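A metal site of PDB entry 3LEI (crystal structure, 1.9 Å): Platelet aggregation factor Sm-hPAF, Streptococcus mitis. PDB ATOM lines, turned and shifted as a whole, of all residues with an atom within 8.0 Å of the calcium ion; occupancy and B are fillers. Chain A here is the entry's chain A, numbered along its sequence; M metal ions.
The calcium ion is bound by O of Arg 31, O of Asn 36, O of Ala 139, OG of Ser 45, OE1 of Glu 140, OD1 of Asp 34 and O of Ser 45.
Six residues have an atom within 4 Å of the calcium ion: Arg 31, Asp 34, Asn 36, Ser 45, Ala 139 and Glu 140.
The nearest printed residue that does not touch the calcium ion is Ala 32 (4.2 Å).
The guanidinium group of Arg 31 sits at hydrogen-bond distance from the backbone carbonyl oxygen of His 44 (3.3 Å).
The side-chain amide oxygen of Asn 36 lies within hydrogen-bond range of the backbone NH of Asp 38 (2.8 Å).
N of Ala 139 is in hydrogen-bond range of O of Tyr 73 (2.8 Å).
The backbone NH (N) of Gly 35 is in hydrogen-bond range of the side-chain carboxylate (OE2) of Glu 140 (2.9 Å).
The backbone carbonyl oxygen (O) of Glu 140 sits at hydrogen-bond distance from the backbone NH (N) of Tyr 73, at 2.8 Å.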
ATOM      1  N   ALA A  28       8.760   3.356 -15.879  1.00  0.00           N
ATOM      2  CA  ALA A  28       7.854   3.325 -14.700  1.00  0.00           C
ATOM      3  C   ALA A  28       8.583   3.523 -13.364  1.00  0.00           C
ATOM      4  O   ALA A  28       9.621   2.943 -13.132  1.00  0.00           O
ATOM      5  CB  ALA A  28       7.027   1.997 -14.679  1.00  0.00           C
ATOM      6  N   ALA A  29       7.991   4.329 -12.487  1.00  0.00           N
ATOM      7  CA  ALA A  29       8.587   4.674 -11.201  1.00  0.00           C
ATOM      8  C   ALA A  29       8.834   3.426 -10.342  1.00  0.00           C
ATOM      9  O   ALA A  29       9.747   3.401  -9.521  1.00  0.00           O
ATOM     10  CB  ALA A  29       7.666   5.630 -10.477  1.00  0.00           C
ATOM     11  N   THR A  30       8.016   2.389 -10.534  1.00  0.00           N
ATOM     12  CA  THR A  30       8.087   1.176  -9.756  1.00  0.00           C
ATOM     13  C   THR A  30       9.360   0.369 -10.077  1.00  0.00           C
ATOM     14  O   THR A  30       9.720  -0.536  -9.332  1.00  0.00           O
ATOM     15  CB  THR A  30       6.816   0.307  -9.957  1.00  0.00           C
ATOM     16  OG1 THR A  30       6.590   0.112 -11.352  1.00  0.00           O
ATOM     17  CG2 THR A  30       5.594   0.957  -9.339  1.00  0.00           C
ATOM     18  N   ARG A  31      10.057   0.706 -11.174  1.00  0.00           N
ATOM     19  CA  ARG A  31      11.324   0.036 -11.531  1.00  0.00           C
ATOM     20  C   ARG A  31      12.454   0.293 -10.562  1.00  0.00           C
ATOM     21  O   ARG A  31      13.385  -0.501 -10.512  1.00  0.00           O
ATOM     22  CB  ARG A  31      11.802   0.494 -12.914  1.00  0.00           C
ATOM     23  CG  ARG A  31      11.087  -0.225 -14.044  1.00  0.00           C
ATOM     24  CD  ARG A  31      11.268   0.519 -15.368  1.00  0.00           C
ATOM     25  NE  ARG A  31      10.432  -0.065 -16.431  1.00  0.00           N
ATOM     26  CZ  ARG A  31      10.735  -0.008 -17.745  1.00  0.00           C
ATOM     27  NH1 ARG A  31       9.917  -0.580 -18.612  1.00  0.00           N
ATOM     28  NH2 ARG A  31      11.816   0.634 -18.183  1.00  0.00           N
ATOM     29  N   ALA A  32      12.371   1.378  -9.806  1.00  0.00           N
ATOM     30  CA  ALA A  32      13.349   1.647  -8.777  1.00  0.00           C
ATOM     31  C   ALA A  32      13.151   0.831  -7.452  1.00  0.00           C
ATOM     32  O   ALA A  32      13.984   0.894  -6.546  1.00  0.00           O
ATOM     33  CB  ALA A  32      13.431   3.219  -8.461  1.00  0.00           C
ATOM     34  N   VAL A  33      12.051   0.108  -7.337  1.00  0.00           N
ATOM     35  CA  VAL A  33      11.740  -0.632  -6.115  1.00  0.00           C
ATOM     36  C   VAL A  33      11.347  -2.057  -6.457  1.00  0.00           C
ATOM     37  O   VAL A  33      10.600  -2.684  -5.695  1.00  0.00           O
ATOM     38  CB  VAL A  33      10.698   0.079  -5.181  1.00  0.00           C
ATOM     39  CG1 VAL A  33      11.343   1.381  -4.529  1.00  0.00           C
ATOM     40  CG2 VAL A  33       9.333   0.310  -5.882  1.00  0.00           C
ATOM     41  N   ASP A  34      11.895  -2.576  -7.573  1.00  0.00           N
ATOM     42  CA  ASP A  34      11.478  -3.884  -8.099  1.00  0.00           C
ATOM     43  C   ASP A  34      12.441  -5.001  -7.654  1.00  0.00           C
ATOM     44  O   ASP A  34      12.271  -6.162  -8.025  1.00  0.00           O
ATOM     45  CB  ASP A  34      11.255  -3.883  -9.628  1.00  0.00           C
ATOM     46  CG  ASP A  34      12.541  -3.635 -10.430  1.00  0.00           C
ATOM     47  OD1 ASP A  34      13.610  -3.306  -9.863  1.00  0.00           O
ATOM     48  OD2 ASP A  34      12.497  -3.735 -11.686  1.00  0.00           O
ATOM     49  N   GLY A  35      13.418  -4.660  -6.825  1.00  0.00           N
ATOM     50  CA  GLY A  35      14.386  -5.634  -6.324  1.00  0.00           C
ATOM     51  C   GLY A  35      15.433  -5.994  -7.355  1.00  0.00           C
ATOM     52  O   GLY A  35      16.021  -7.062  -7.278  1.00  0.00           O
ATOM     53  N   ASN A  36      15.671  -5.122  -8.329  1.00  0.00           N
ATOM     54  CA  ASN A  36      16.665  -5.399  -9.379  1.00  0.00           C
ATOM     55  C   ASN A  36      17.518  -4.124  -9.588  1.00  0.00           C
ATOM     56  O   ASN A  36      17.016  -3.085 -10.054  1.00  0.00           O
ATOM     57  CB  ASN A  36      15.947  -5.827 -10.674  1.00  0.00           C
ATOM     58  CG  ASN A  36      16.932  -6.222 -11.801  1.00  0.00           C
ATOM     59  OD1 ASN A  36      18.170  -6.037 -11.687  1.00  0.00           O
ATOM     60  ND2 ASN A  36      16.394  -6.754 -12.893  1.00  0.00           N
ATOM     61  N   VAL A  37      18.798  -4.194  -9.208  1.00  0.00           N
ATOM     62  CA  VAL A  37      19.683  -3.054  -9.368  1.00  0.00           C
ATOM     63  C   VAL A  37      20.356  -2.980 -10.767  1.00  0.00           C
ATOM     64  O   VAL A  37      21.200  -2.132 -10.973  1.00  0.00           O
ATOM     65  CB  VAL A  37      20.812  -3.056  -8.304  1.00  0.00           C
ATOM     66  CG1 VAL A  37      20.248  -3.149  -6.850  1.00  0.00           C
ATOM     67  CG2 VAL A  37      21.759  -4.227  -8.570  1.00  0.00           C
ATOM     68  N   ASP A  38      20.025  -3.890 -11.688  1.00  0.00           N
ATOM     69  CA  ASP A  38      20.566  -3.823 -13.063  1.00  0.00           C
ATOM     70  C   ASP A  38      20.405  -2.399 -13.643  1.00  0.00           C
ATOM     71  O   ASP A  38      19.282  -1.905 -13.818  1.00  0.00           O
ATOM     72  CB  ASP A  38      19.789  -4.766 -13.997  1.00  0.00           C
ATOM     73  CG  ASP A  38      20.505  -5.001 -15.313  1.00  0.00           C
ATOM     74  OD1 ASP A  38      20.387  -6.140 -15.796  1.00  0.00           O
ATOM     75  OD2 ASP A  38      21.185  -4.083 -15.867  1.00  0.00           O
ATOM     76  N   SER A  39      21.525  -1.752 -13.951  1.00  0.00           N
ATOM     77  CA  SER A  39      21.500  -0.334 -14.275  1.00  0.00           C
ATOM     78  C   SER A  39      21.418  -0.058 -15.802  1.00  0.00           C
ATOM     79  O   SER A  39      21.544   1.086 -16.232  1.00  0.00           O
ATOM     80  CB  SER A  39      22.763   0.321 -13.711  1.00  0.00           C
ATOM     81  OG  SER A  39      23.893  -0.123 -14.478  1.00  0.00           O
ATOM     82  N   HIS A  43      17.347  -3.161 -20.062  1.00  0.00           N
ATOM     83  CA  HIS A  43      16.943  -4.309 -19.252  1.00  0.00           C
ATOM     84  C   HIS A  43      15.678  -4.029 -18.403  1.00  0.00           C
ATOM     85  O   HIS A  43      15.261  -4.870 -17.597  1.00  0.00           O
ATOM     86  CB  HIS A  43      18.126  -4.813 -18.375  1.00  0.00           C
ATOM     87  CG  HIS A  43      19.294  -5.298 -19.190  1.00  0.00           C
ATOM     88  ND1 HIS A  43      20.504  -5.659 -18.634  1.00  0.00           N
ATOM     89  CD2 HIS A  43      19.424  -5.507 -20.538  1.00  0.00           C
ATOM     90  CE1 HIS A  43      21.340  -6.028 -19.591  1.00  0.00           C
ATOM     91  NE2 HIS A  43      20.704  -5.950 -20.752  1.00  0.00           N
ATOM     92  N   HIS A  44      15.106  -2.831 -18.583  1.00  0.00           N
ATOM     93  CA  HIS A  44      13.768  -2.503 -18.107  1.00  0.00           C
ATOM     94  C   HIS A  44      13.645  -2.365 -16.596  1.00  0.00           C
ATOM     95  O   HIS A  44      12.541  -2.537 -16.055  1.00  0.00           O
ATOM     96  CB  HIS A  44      12.734  -3.565 -18.613  1.00  0.00           C
ATOM     97  CG  HIS A  44      12.682  -3.712 -20.103  1.00  0.00           C
ATOM     98  ND1 HIS A  44      12.672  -2.637 -20.962  1.00  0.00           N
ATOM     99  CD2 HIS A  44      12.639  -4.827 -20.892  1.00  0.00           C
ATOM    100  CE1 HIS A  44      12.608  -3.072 -22.209  1.00  0.00           C
ATOM    101  NE2 HIS A  44      12.571  -4.406 -22.194  1.00  0.00           N
ATOM    102  N   SER A  45      14.741  -2.080 -15.892  1.00  0.00           N
ATOM    103  CA  SER A  45      14.675  -1.948 -14.432  1.00  0.00           C
ATOM    104  C   SER A  45      15.156  -0.568 -13.916  1.00  0.00           C
ATOM    105  O   SER A  45      15.522  -0.425 -12.716  1.00  0.00           O
ATOM    106  CB  SER A  45      15.414  -3.088 -13.697  1.00  0.00           C
ATOM    107  OG  SER A  45      14.925  -3.159 -12.360  1.00  0.00           O
ATOM    108  N   VAL A  46      15.157   0.408 -14.827  1.00  0.00           N
ATOM    109  CA  VAL A  46      15.591   1.770 -14.537  1.00  0.00           C
ATOM    110  C   VAL A  46      14.421   2.714 -14.910  1.00  0.00           C
ATOM    111  O   VAL A  46      13.763   2.532 -15.929  1.00  0.00           O
ATOM    112  CB  VAL A  46      16.859   2.159 -15.350  1.00  0.00           C
ATOM    113  CG1 VAL A  46      17.309   3.607 -15.063  1.00  0.00           C
ATOM    114  CG2 VAL A  46      17.985   1.143 -15.179  1.00  0.00           C
ATOM    115  N   THR A  47      14.166   3.696 -14.050  1.00  0.00           N
ATOM    116  CA  THR A  47      13.083   4.647 -14.232  1.00  0.00           C
ATOM    117  C   THR A  47      13.501   5.745 -15.203  1.00  0.00           C
ATOM    118  O   THR A  47      14.676   5.813 -15.570  1.00  0.00           O
ATOM    119  CB  THR A  47      12.689   5.318 -12.855  1.00  0.00           C
ATOM    120  OG1 THR A  47      13.717   6.234 -12.476  1.00  0.00           O
ATOM    121  CG2 THR A  47      12.484   4.281 -11.734  1.00  0.00           C
ATOM    122  N   TYR A  73      20.974   3.635  -6.736  1.00  0.00           N
ATOM    123  CA  TYR A  73      21.729   2.976  -7.822  1.00  0.00           C
ATOM    124  C   TYR A  73      21.488   3.746  -9.100  1.00  0.00           C
ATOM    125  O   TYR A  73      20.352   3.876  -9.536  1.00  0.00           O
ATOM    126  CB  TYR A  73      21.267   1.533  -8.013  1.00  0.00           C
ATOM    127  CG  TYR A  73      21.592   0.681  -6.826  1.00  0.00           C
ATOM    128  CD1 TYR A  73      22.711  -0.149  -6.816  1.00  0.00           C
ATOM    129  CD2 TYR A  73      20.782   0.696  -5.694  1.00  0.00           C
ATOM    130  CE1 TYR A  73      22.999  -0.951  -5.724  1.00  0.00           C
ATOM    131  CE2 TYR A  73      21.054  -0.077  -4.598  1.00  0.00           C
ATOM    132  CZ  TYR A  73      22.155  -0.905  -4.620  1.00  0.00           C
ATOM    133  OH  TYR A  73      22.370  -1.693  -3.518  1.00  0.00           O
ATOM    134  N   LEU A 138      16.590   6.280 -12.135  1.00  0.00           N
ATOM    135  CA  LEU A 138      17.157   5.522 -11.033  1.00  0.00           C
ATOM    136  C   LEU A 138      17.055   4.014 -11.343  1.00  0.00           C
ATOM    137  O   LEU A 138      15.967   3.506 -11.645  1.00  0.00           O
ATOM    138  CB  LEU A 138      16.391   5.844  -9.744  1.00  0.00           C
ATOM    139  CG  LEU A 138      16.575   7.294  -9.245  1.00  0.00           C
ATOM    140  CD1 LEU A 138      15.422   7.786  -8.322  1.00  0.00           C
ATOM    141  CD2 LEU A 138      17.940   7.441  -8.592  1.00  0.00           C
ATOM    142  N   ALA A 139      18.169   3.291 -11.175  1.00  0.00           N
ATOM    143  CA  ALA A 139      18.154   1.839 -11.348  1.00  0.00           C
ATOM    144  C   ALA A 139      17.415   1.214 -10.156  1.00  0.00           C
ATOM    145  O   ALA A 139      16.701   0.227 -10.320  1.00  0.00           O
ATOM    146  CB  ALA A 139      19.611   1.267 -11.491  1.00  0.00           C
ATOM    147  N   GLU A 140      17.611   1.792  -8.982  1.00  0.00           N
ATOM    148  CA  GLU A 140      17.042   1.255  -7.743  1.00  0.00           C
ATOM    149  C   GLU A 140      17.253   2.236  -6.604  1.00  0.00           C
ATOM    150  O   GLU A 140      18.247   2.977  -6.566  1.00  0.00           O
ATOM    151  CB  GLU A 140      17.639  -0.129  -7.369  1.00  0.00           C
ATOM    152  CG  GLU A 140      16.865  -0.909  -6.309  1.00  0.00           C
ATOM    153  CD  GLU A 140      15.640  -1.682  -6.864  1.00  0.00           C
ATOM    154  OE1 GLU A 140      15.299  -1.582  -8.067  1.00  0.00           O
ATOM    155  OE2 GLU A 140      15.001  -2.396  -6.079  1.00  0.00           O
ATOM    156  N   VAL A 141      16.277   2.271  -5.711  1.00  0.00           N
ATOM    157  CA  VAL A 141      16.387   2.949  -4.417  1.00  0.00           C
ATOM    158  C   VAL A 141      16.097   1.927  -3.331  1.00  0.00           C
ATOM    159  O   VAL A 141      15.022   1.307  -3.312  1.00  0.00           O
ATOM    160  CB  VAL A 141      15.442   4.178  -4.307  1.00  0.00           C
ATOM    161  CG1 VAL A 141      15.549   4.835  -2.909  1.00  0.00           C
ATOM    162  CG2 VAL A 141      15.753   5.188  -5.437  1.00  0.00           C
HETATM  163 CA    CA M   1      15.319  -1.631 -10.530  1.00  0.00          CA
